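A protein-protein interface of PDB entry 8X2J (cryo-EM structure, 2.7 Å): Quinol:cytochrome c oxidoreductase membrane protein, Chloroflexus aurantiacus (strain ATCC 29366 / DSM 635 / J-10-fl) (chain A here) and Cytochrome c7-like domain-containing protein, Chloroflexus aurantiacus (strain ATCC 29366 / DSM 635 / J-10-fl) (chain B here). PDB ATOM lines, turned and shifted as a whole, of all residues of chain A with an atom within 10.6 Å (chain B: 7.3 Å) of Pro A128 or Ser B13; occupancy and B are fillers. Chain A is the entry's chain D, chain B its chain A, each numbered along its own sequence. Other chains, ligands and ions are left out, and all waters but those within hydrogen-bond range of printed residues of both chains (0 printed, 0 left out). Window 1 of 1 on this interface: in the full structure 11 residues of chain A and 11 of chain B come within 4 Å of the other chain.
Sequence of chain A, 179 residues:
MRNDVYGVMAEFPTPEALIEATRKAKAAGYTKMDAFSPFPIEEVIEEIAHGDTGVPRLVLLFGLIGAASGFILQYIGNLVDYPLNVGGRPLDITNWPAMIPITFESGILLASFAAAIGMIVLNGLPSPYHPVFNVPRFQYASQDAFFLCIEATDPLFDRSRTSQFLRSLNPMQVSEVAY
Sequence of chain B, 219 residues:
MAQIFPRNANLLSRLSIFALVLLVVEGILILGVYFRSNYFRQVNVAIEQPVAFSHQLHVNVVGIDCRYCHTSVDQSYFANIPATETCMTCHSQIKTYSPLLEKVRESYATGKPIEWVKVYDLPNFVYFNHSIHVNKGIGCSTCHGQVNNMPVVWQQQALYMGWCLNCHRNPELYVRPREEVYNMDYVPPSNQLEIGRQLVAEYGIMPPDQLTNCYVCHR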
ATOM      1  N   ILE A 120      39.072  16.946   9.859  1.00  0.00           N
ATOM      2  CA  ILE A 120      37.787  16.785   9.174  1.00  0.00           C
ATOM      3  C   ILE A 120      37.572  15.333   8.754  1.00  0.00           C
ATOM      4  O   ILE A 120      36.484  14.775   8.938  1.00  0.00           O
ATOM      5  CB  ILE A 120      37.703  17.747   7.968  1.00  0.00           C
ATOM      6  CG1 ILE A 120      37.720  19.216   8.405  1.00  0.00           C
ATOM      7  CG2 ILE A 120      36.456  17.508   7.150  1.00  0.00           C
ATOM      8  CD1 ILE A 120      36.817  19.555   9.543  1.00  0.00           C
ATOM      9  N   ASN A 123      37.584  12.812  12.253  1.00  0.00           N
ATOM     10  CA  ASN A 123      36.353  12.825  13.088  1.00  0.00           C
ATOM     11  C   ASN A 123      35.184  12.335  12.230  1.00  0.00           C
ATOM     12  O   ASN A 123      34.091  12.139  12.786  1.00  0.00           O
ATOM     13  CB  ASN A 123      36.085  14.201  13.706  1.00  0.00           C
ATOM     14  CG  ASN A 123      35.751  15.262  12.680  1.00  0.00           C
ATOM     15  OD1 ASN A 123      35.858  15.027  11.479  1.00  0.00           O
ATOM     16  ND2 ASN A 123      35.348  16.434  13.143  1.00  0.00           N
ATOM     17  N   GLY A 124      35.417  12.129  10.931  1.00  0.00           N
ATOM     18  CA  GLY A 124      34.330  11.719  10.022  1.00  0.00           C
ATOM     19  C   GLY A 124      33.310  12.832   9.859  1.00  0.00           C
ATOM     20  O   GLY A 124      32.117  12.518   9.677  1.00  0.00           O
ATOM     21  N   LEU A 125      33.763  14.088   9.923  1.00  0.00           N
ATOM     22  CA  LEU A 125      32.844  15.254   9.800  1.00  0.00           C
ATOM     23  C   LEU A 125      32.144  15.257   8.433  1.00  0.00           C
ATOM     24  O   LEU A 125      30.957  15.625   8.407  1.00  0.00           O
ATOM     25  CB  LEU A 125      33.631  16.551  10.011  1.00  0.00           C
ATOM     26  CG  LEU A 125      32.776  17.817  10.066  1.00  0.00           C
ATOM     27  CD1 LEU A 125      31.659  17.666  11.087  1.00  0.00           C
ATOM     28  CD2 LEU A 125      33.626  19.036  10.389  1.00  0.00           C
ATOM     29  N   PRO A 126      32.796  14.892   7.302  1.00  0.00           N
ATOM     30  CA  PRO A 126      32.161  14.977   5.978  1.00  0.00           C
ATOM     31  C   PRO A 126      30.938  14.057   5.849  1.00  0.00           C
ATOM     32  O   PRO A 126      30.850  13.344   4.865  1.00  0.00           O
ATOM     33  CB  PRO A 126      33.251  14.503   5.005  1.00  0.00           C
ATOM     34  CG  PRO A 126      34.541  14.718   5.759  1.00  0.00           C
ATOM     35  CD  PRO A 126      34.182  14.428   7.200  1.00  0.00           C
ATOM     36  N   SER A 127      30.034  14.096   6.831  1.00  0.00           N
ATOM     37  CA  SER A 127      28.787  13.290   6.776  1.00  0.00           C
ATOM     38  C   SER A 127      27.609  14.189   7.158  1.00  0.00           C
ATOM     39  O   SER A 127      27.032  13.979   8.245  1.00  0.00           O
ATOM     40  CB  SER A 127      28.881  12.090   7.679  1.00  0.00           C
ATOM     41  OG  SER A 127      29.193  12.484   9.008  1.00  0.00           O
ATOM     42  N   PRO A 128      27.228  15.181   6.322  1.00  0.00           N
ATOM     43  CA  PRO A 128      26.162  16.120   6.680  1.00  0.00           C
ATOM     44  C   PRO A 128      24.909  15.357   7.124  1.00  0.00           C
ATOM     45  O   PRO A 128      24.342  15.712   8.141  1.00  0.00           O
ATOM     46  CB  PRO A 128      25.895  16.865   5.366  1.00  0.00           C
ATOM     47  CG  PRO A 128      27.215  16.795   4.629  1.00  0.00           C
ATOM     48  CD  PRO A 128      27.792  15.444   4.996  1.00  0.00           C
ATOM     49  N   TYR A 129      24.520  14.329   6.364  1.00  0.00           N
ATOM     50  CA  TYR A 129      23.355  13.495   6.757  1.00  0.00           C
ATOM     51  C   TYR A 129      23.802  12.470   7.802  1.00  0.00           C
ATOM     52  O   TYR A 129      24.560  11.547   7.448  1.00  0.00           O
ATOM     53  CB  TYR A 129      22.741  12.799   5.540  1.00  0.00           C
ATOM     54  CG  TYR A 129      21.643  11.823   5.877  1.00  0.00           C
ATOM     55  CD1 TYR A 129      21.928  10.497   6.154  1.00  0.00           C
ATOM     56  CD2 TYR A 129      20.319  12.225   5.931  1.00  0.00           C
ATOM     57  CE1 TYR A 129      20.928   9.594   6.473  1.00  0.00           C
ATOM     58  CE2 TYR A 129      19.306  11.334   6.241  1.00  0.00           C
ATOM     59  CZ  TYR A 129      19.610  10.013   6.514  1.00  0.00           C
ATOM     60  OH  TYR A 129      18.619   9.128   6.824  1.00  0.00           O
ATOM     61  N   HIS A 130      23.353  12.634   9.049  1.00  0.00           N
ATOM     62  CA  HIS A 130      23.692  11.689  10.094  1.00  0.00           C
ATOM     63  C   HIS A 130      22.387  11.143  10.645  1.00  0.00           C
ATOM     64  O   HIS A 130      21.354  11.820  10.566  1.00  0.00           O
ATOM     65  CB  HIS A 130      24.517  12.334  11.218  1.00  0.00           C
ATOM     66  CG  HIS A 130      25.347  11.357  11.990  1.00  0.00           C
ATOM     67  ND1 HIS A 130      24.908  10.767  13.155  1.00  0.00           N
ATOM     68  CD2 HIS A 130      26.578  10.847  11.753  1.00  0.00           C
ATOM     69  CE1 HIS A 130      25.837   9.948  13.611  1.00  0.00           C
ATOM     70  NE2 HIS A 130      26.861   9.978  12.778  1.00  0.00           N
ATOM     71  N   PRO A 131      22.388   9.909  11.160  1.00  0.00           N
ATOM     72  CA  PRO A 131      21.184   9.394  11.831  1.00  0.00           C
ATOM     73  C   PRO A 131      20.753  10.201  13.043  1.00  0.00           C
ATOM     74  O   PRO A 131      19.561  10.200  13.359  1.00  0.00           O
ATOM     75  CB  PRO A 131      21.594   7.972  12.226  1.00  0.00           C
ATOM     76  CG  PRO A 131      22.565   7.577  11.188  1.00  0.00           C
ATOM     77  CD  PRO A 131      23.322   8.822  10.818  1.00  0.00           C
ATOM     78  N   VAL A 132      21.672  10.920  13.696  1.00  0.00           N
ATOM     79  CA  VAL A 132      21.377  11.624  14.939  1.00  0.00           C
ATOM     80  C   VAL A 132      20.429  12.809  14.734  1.00  0.00           C
ATOM     81  O   VAL A 132      19.779  13.250  15.688  1.00  0.00           O
ATOM     82  CB  VAL A 132      22.711  12.053  15.591  1.00  0.00           C
ATOM     83  CG1 VAL A 132      23.317  13.257  14.888  1.00  0.00           C
ATOM     84  CG2 VAL A 132      22.556  12.301  17.069  1.00  0.00           C
ATOM     85  N   PHE A 133      20.293  13.312  13.506  1.00  0.00           N
ATOM     86  CA  PHE A 133      19.388  14.420  13.230  1.00  0.00           C
ATOM     87  C   PHE A 133      17.937  13.980  13.080  1.00  0.00           C
ATOM     88  O   PHE A 133      17.065  14.837  12.907  1.00  0.00           O
ATOM     89  CB  PHE A 133      19.827  15.160  11.965  1.00  0.00           C
ATOM     90  CG  PHE A 133      21.130  15.892  12.107  1.00  0.00           C
ATOM     91  CD1 PHE A 133      21.248  16.960  12.981  1.00  0.00           C
ATOM     92  CD2 PHE A 133      22.234  15.521  11.356  1.00  0.00           C
ATOM     93  CE1 PHE A 133      22.444  17.641  13.108  1.00  0.00           C
ATOM     94  CE2 PHE A 133      23.433  16.196  11.479  1.00  0.00           C
ATOM     95  CZ  PHE A 133      23.537  17.258  12.356  1.00  0.00           C
ATOM     96  N   ASN A 134      17.662  12.673  13.132  1.00  0.00           N
ATOM     97  CA  ASN A 134      16.293  12.178  13.043  1.00  0.00           C
ATOM     98  C   ASN A 134      15.464  12.537  14.268  1.00  0.00           C
ATOM     99  O   ASN A 134      14.231  12.567  14.178  1.00  0.00           O
ATOM    100  CB  ASN A 134      16.298  10.662  12.851  1.00  0.00           C
ATOM    101  CG  ASN A 134      16.531  10.259  11.413  1.00  0.00           C
ATOM    102  OD1 ASN A 134      15.812  10.689  10.512  1.00  0.00           O
ATOM    103  ND2 ASN A 134      17.547   9.437  11.185  1.00  0.00           N
ATOM    104  N   PHE A 138      16.827  17.465  18.299  1.00  0.00           N
ATOM    105  CA  PHE A 138      18.256  17.642  18.070  1.00  0.00           C
ATOM    106  C   PHE A 138      18.581  18.952  17.363  1.00  0.00           C
ATOM    107  O   PHE A 138      19.762  19.270  17.189  1.00  0.00           O
ATOM    108  CB  PHE A 138      18.819  16.465  17.266  1.00  0.00           C
ATOM    109  CG  PHE A 138      20.284  16.218  17.502  1.00  0.00           C
ATOM    110  CD1 PHE A 138      20.726  15.697  18.707  1.00  0.00           C
ATOM    111  CD2 PHE A 138      21.219  16.530  16.528  1.00  0.00           C
ATOM    112  CE1 PHE A 138      22.073  15.479  18.930  1.00  0.00           C
ATOM    113  CE2 PHE A 138      22.566  16.319  16.746  1.00  0.00           C
ATOM    114  CZ  PHE A 138      22.992  15.793  17.947  1.00  0.00           C
ATOM    115  N   ALA B   2      19.628  14.520   8.584  1.00  0.00           N
ATOM    116  CA  ALA B   2      18.364  13.801   8.502  1.00  0.00           C
ATOM    117  C   ALA B   2      17.191  14.756   8.635  1.00  0.00           C
ATOM    118  O   ALA B   2      16.103  14.500   8.119  1.00  0.00           O
ATOM    119  CB  ALA B   2      18.296  12.730   9.566  1.00  0.00           C
ATOM    120  N   GLN B   3      17.421  15.860   9.343  1.00  0.00           N
ATOM    121  CA  GLN B   3      16.380  16.870   9.482  1.00  0.00           C
ATOM    122  C   GLN B   3      16.202  17.654   8.188  1.00  0.00           C
ATOM    123  O   GLN B   3      15.079  18.019   7.825  1.00  0.00           O
ATOM    124  CB  GLN B   3      16.719  17.806  10.643  1.00  0.00           C
ATOM    125  CG  GLN B   3      15.591  18.741  11.047  1.00  0.00           C
ATOM    126  CD  GLN B   3      14.400  17.999  11.619  1.00  0.00           C
ATOM    127  OE1 GLN B   3      13.376  17.836  10.954  1.00  0.00           O
ATOM    128  NE2 GLN B   3      14.528  17.542  12.858  1.00  0.00           N
ATOM    129  N   PHE B   5      18.984  17.547   5.114  1.00  0.00           N
ATOM    130  CA  PHE B   5      19.625  16.915   3.975  1.00  0.00           C
ATOM    131  C   PHE B   5      19.150  15.471   3.815  1.00  0.00           C
ATOM    132  O   PHE B   5      18.827  14.804   4.802  1.00  0.00           O
ATOM    133  CB  PHE B   5      21.138  16.956   4.153  1.00  0.00           C
ATOM    134  CG  PHE B   5      21.724  18.323   3.983  1.00  0.00           C
ATOM    135  CD1 PHE B   5      22.046  18.801   2.724  1.00  0.00           C
ATOM    136  CD2 PHE B   5      21.951  19.132   5.083  1.00  0.00           C
ATOM    137  CE1 PHE B   5      22.587  20.060   2.568  1.00  0.00           C
ATOM    138  CE2 PHE B   5      22.494  20.391   4.933  1.00  0.00           C
ATOM    139  CZ  PHE B   5      22.810  20.855   3.674  1.00  0.00           C
ATOM    140  N   PRO B   6      19.095  14.953   2.570  1.00  0.00           N
ATOM    141  CA  PRO B   6      18.654  13.564   2.381  1.00  0.00           C
ATOM    142  C   PRO B   6      19.755  12.554   2.657  1.00  0.00           C
ATOM    143  O   PRO B   6      20.844  12.923   3.103  1.00  0.00           O
ATOM    144  CB  PRO B   6      18.209  13.522   0.912  1.00  0.00           C
ATOM    145  CG  PRO B   6      18.659  14.800   0.290  1.00  0.00           C
ATOM    146  CD  PRO B   6      19.400  15.613   1.290  1.00  0.00           C
ATOM    147  N   ASN B   8      21.574  10.563   0.639  1.00  0.00           N
ATOM    148  CA  ASN B   8      22.734  10.574  -0.246  1.00  0.00           C
ATOM    149  C   ASN B   8      23.532  11.873  -0.183  1.00  0.00           C
ATOM    150  O   ASN B   8      24.374  12.103  -1.059  1.00  0.00           O
ATOM    151  CB  ASN B   8      22.298  10.308  -1.690  1.00  0.00           C
ATOM    152  CG  ASN B   8      21.079  11.113  -2.088  1.00  0.00           C
ATOM    153  OD1 ASN B   8      20.472  11.793  -1.262  1.00  0.00           O
ATOM    154  ND2 ASN B   8      20.713  11.041  -3.361  1.00  0.00           N
ATOM    155  N   ALA B   9      23.298  12.717   0.825  1.00  0.00           N
ATOM    156  CA  ALA B   9      24.013  13.984   0.919  1.00  0.00           C
ATOM    157  C   ALA B   9      25.477  13.789   1.290  1.00  0.00           C
ATOM    158  O   ALA B   9      26.321  14.591   0.881  1.00  0.00           O
ATOM    159  CB  ALA B   9      23.330  14.903   1.928  1.00  0.00           C
ATOM    160  N   ASN B  10      25.801  12.735   2.048  1.00  0.00           N
ATOM    161  CA  ASN B  10      27.193  12.469   2.409  1.00  0.00           C
ATOM    162  C   ASN B  10      28.011  12.067   1.188  1.00  0.00           C
ATOM    163  O   ASN B  10      29.104  12.603   0.952  1.00  0.00           O
ATOM    164  CB  ASN B  10      27.260  11.372   3.468  1.00  0.00           C
ATOM    165  CG  ASN B  10      26.252  11.570   4.566  1.00  0.00           C
ATOM    166  OD1 ASN B  10      25.897  12.697   4.887  1.00  0.00           O
ATOM    167  ND2 ASN B  10      25.791  10.476   5.158  1.00  0.00           N
ATOM    168  N   LEU B  11      27.485  11.122   0.405  1.00  0.00           N
ATOM    169  CA  LEU B  11      28.117  10.720  -0.846  1.00  0.00           C
ATOM    170  C   LEU B  11      28.167  11.873  -1.835  1.00  0.00           C
ATOM    171  O   LEU B  11      29.167  12.036  -2.541  1.00  0.00           O
ATOM    172  CB  LEU B  11      27.364   9.528  -1.440  1.00  0.00           C
ATOM    173  CG  LEU B  11      27.654   9.081  -2.873  1.00  0.00           C
ATOM    174  CD1 LEU B  11      29.091   8.625  -3.013  1.00  0.00           C
ATOM    175  CD2 LEU B  11      26.699   7.974  -3.278  1.00  0.00           C
ATOM    176  N   LEU B  12      27.117  12.700  -1.868  1.00  0.00           N
ATOM    177  CA  LEU B  12      27.095  13.859  -2.754  1.00  0.00           C
ATOM    178  C   LEU B  12      28.152  14.886  -2.363  1.00  0.00           C
ATOM    179  O   LEU B  12      28.810  15.459  -3.235  1.00  0.00           O
ATOM    180  CB  LEU B  12      25.704  14.486  -2.748  1.00  0.00           C
ATOM    181  CG  LEU B  12      25.338  15.322  -3.970  1.00  0.00           C
ATOM    182  CD1 LEU B  12      25.295  14.441  -5.204  1.00  0.00           C
ATOM    183  CD2 LEU B  12      24.005  16.021  -3.756  1.00  0.00           C
ATOM    184  N   SER B  13      28.356  15.109  -1.062  1.00  0.00           N
ATOM    185  CA  SER B  13      29.355  16.074  -0.611  1.00  0.00           C
ATOM    186  C   SER B  13      30.774  15.570  -0.847  1.00  0.00           C
ATOM    187  O   SER B  13      31.654  16.343  -1.255  1.00  0.00           O
ATOM    188  CB  SER B  13      29.141  16.388   0.866  1.00  0.00           C
ATOM    189  OG  SER B  13      27.890  17.017   1.065  1.00  0.00           O
ATOM    190  N   ARG B  14      31.016  14.279  -0.591  1.00  0.00           N
ATOM    191  CA  ARG B  14      32.335  13.705  -0.852  1.00  0.00           C
ATOM    192  C   ARG B  14      32.652  13.700  -2.344  1.00  0.00           C
ATOM    193  O   ARG B  14      33.772  14.041  -2.753  1.00  0.00           O
ATOM    194  CB  ARG B  14      32.409  12.292  -0.282  1.00  0.00           C
ATOM    195  CG  ARG B  14      32.484  12.245   1.227  1.00  0.00           C
ATOM    196  CD  ARG B  14      31.871  10.968   1.756  1.00  0.00           C
ATOM    197  NE  ARG B  14      31.359  11.127   3.110  1.00  0.00           N
ATOM    198  CZ  ARG B  14      30.638  10.213   3.745  1.00  0.00           C
ATOM    199  NH1 ARG B  14      30.311   9.069   3.169  1.00  0.00           N
ATOM    200  NH2 ARG B  14      30.237  10.454   4.989  1.00  0.00           N
ATOM    201  N   LEU B  15      31.664  13.351  -3.173  1.00  0.00           N
ATOM    202  CA  LEU B  15      31.844  13.383  -4.617  1.00  0.00           C
ATOM    203  C   LEU B  15      31.977  14.811  -5.131  1.00  0.00           C
ATOM    204  O   LEU B  15      32.663  15.040  -6.127  1.00  0.00           O
ATOM    205  CB  LEU B  15      30.673  12.665  -5.291  1.00  0.00           C
ATOM    206  CG  LEU B  15      30.744  12.359  -6.785  1.00  0.00           C
ATOM    207  CD1 LEU B  15      31.900  11.419  -7.078  1.00  0.00           C
ATOM    208  CD2 LEU B  15      29.432  11.760  -7.262  1.00  0.00           C
ATOM    209  N   SER B  16      31.361  15.782  -4.449  1.00  0.00           N
ATOM    210  CA  SER B  16      31.520  17.182  -4.822  1.00  0.00           C
ATOM    211  C   SER B  16      32.926  17.686  -4.530  1.00  0.00           C
ATOM    212  O   SER B  16      33.499  18.423  -5.338  1.00  0.00           O
ATOM    213  CB  SER B  16      30.485  18.035  -4.090  1.00  0.00           C
ATOM    214  OG  SER B  16      30.332  19.297  -4.712  1.00  0.00           O
ATOM    215  N   ILE B  17      33.494  17.301  -3.381  1.00  0.00           N
ATOM    216  CA  ILE B  17      34.880  17.662  -3.064  1.00  0.00           C
ATOM    217  C   ILE B  17      35.842  17.013  -4.057  1.00  0.00           C
ATOM    218  O   ILE B  17      36.771  17.662  -4.568  1.00  0.00           O
ATOM    219  CB  ILE B  17      35.209  17.269  -1.608  1.00  0.00           C
ATOM    220  CG1 ILE B  17      34.390  18.105  -0.621  1.00  0.00           C
ATOM    221  CG2 ILE B  17      36.701  17.398  -1.316  1.00  0.00           C
ATOM    222  CD1 ILE B  17      34.839  19.545  -0.502  1.00  0.00           C
ATOM    223  N   PHE B  18      35.604  15.733  -4.370  1.00  0.00           N
ATOM    224  CA  PHE B  18      36.419  15.008  -5.345  1.00  0.00           C
ATOM    225  C   PHE B  18      36.331  15.631  -6.736  1.00  0.00           C
ATOM    226  O   PHE B  18      37.354  15.812  -7.410  1.00  0.00           O
ATOM    227  CB  PHE B  18      35.967  13.549  -5.382  1.00  0.00           C
ATOM    228  CG  PHE B  18      36.888  12.640  -6.130  1.00  0.00           C
ATOM    229  CD1 PHE B  18      38.189  12.442  -5.698  1.00  0.00           C
ATOM    230  CD2 PHE B  18      36.445  11.966  -7.256  1.00  0.00           C
ATOM    231  CE1 PHE B  18      39.033  11.596  -6.381  1.00  0.00           C
ATOM    232  CE2 PHE B  18      37.286  11.117  -7.945  1.00  0.00           C
ATOM    233  CZ  PHE B  18      38.582  10.932  -7.507  1.00  0.00           C
ATOM    234  N   ALA B  19      35.121  15.999  -7.163  1.00  0.00           N
ATOM    235  CA  ALA B  19      34.930  16.605  -8.473  1.00  0.00           C
ATOM    236  C   ALA B  19      35.485  18.019  -8.531  1.00  0.00           C
ATOM    237  O   ALA B  19      35.941  18.448  -9.590  1.00  0.00           O
ATOM    238  CB  ALA B  19      33.448  16.600  -8.842  1.00  0.00           C
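The backbone carbonyl oxygen (O) of Pro A131 sits at hydrogen-bond distance from the side-chain amide nitrogen (ND2) of Asn A134 (3.1 Å).
O of Gly A124 lies within hydrogen-bond range of OG of Ser A127 (3.0 Å).
The guanidinium group of Arg B14 lies close to the backbone carbonyl oxygen of Asn B10 (3.5 Å).
N of Val A132 sits close to ND1 of His A130 (3.3 Å).
O of Ala B9 sits at hydrogen-bond distance from OG of Ser B13 (2.9 Å).
Asn B10 touches Ser A127.
CB of Ser A127 touches NH2 of Arg B14, at 3.4 Å.
Pro A128 touches Ser B13 (CG to OG, 3.6 Å).
Tyr A129 touches Ala B2 (CE2 to CA, 3.5 Å).
CD2 of Tyr A129 touches O of Phe B5, at 3.2 Å.
O of Pro B6 touches CD2 of Tyr A129, 3.0 Å away.
His A130 touches Ala B2.
Phe A133 touches Ala B2 (CB to N, 3.4 Å).
Phe A133 touches Gln B3.
Ala B2 touches Asn A134.
The backbone nitrogen (N) of Pro A128 lies close to the side-chain amide oxygen (OD1) of Asn B10 (3.2 Å).
The backbone NH (N) of Tyr A129 lies within hydrogen-bond range of the side-chain amide oxygen (OD1) of Asn B10 (2.6 Å).
The guanidinium group (NE) of Arg B14 lies within hydrogen-bond range of the backbone carbonyl oxygen (O) of Pro A126 (2.9 Å).
Pro A128 touches just these residues of chain B: Asn B10 and Ser B13.
Ser B13 touches one residue of chain A.
No residue of chain A comes within 4 Å of Leu B12.
No residue of chain A comes within 4 Å of Ser B16.
No residue of chain A comes within 4 Å of Ile B17.
Of the printed residues of chain B, Tyr A129 touches Ala B2, Phe B5, Pro B6 and Asn B10.
Of the printed residues of chain A, Gln B3 touches Phe A133 (3.6 Å).
Ala B19 touches none of the printed residues of chain A.
Leu B11 touches none of the printed residues of chain A.
The nearest residue of chain A that does not touch Ser B13 is Pro A126 (5.3 Å).
Of the 16 printed residues of chain B, 7 touch a printed residue of chain A.
Printed residues of chain B that touch a printed residue of chain A: Ala B2, Gln B3, Phe B5, Pro B6, Asn B10, Ser B13 and Arg B14.
Hydrophobic or aromatic side chains of chain A that line the printed part of chain B: Pro A128, Tyr A129 and Phe A133.
Along chain A the printed residues that touch a printed residue of chain B span positions 126 to 134.
Among the printed residues, 13 pairs touch across the chains.
Among the printed residues, no Asp or Glu carboxylate lies within 4 Å of a Lys or Arg side-chain nitrogen of the other chain.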
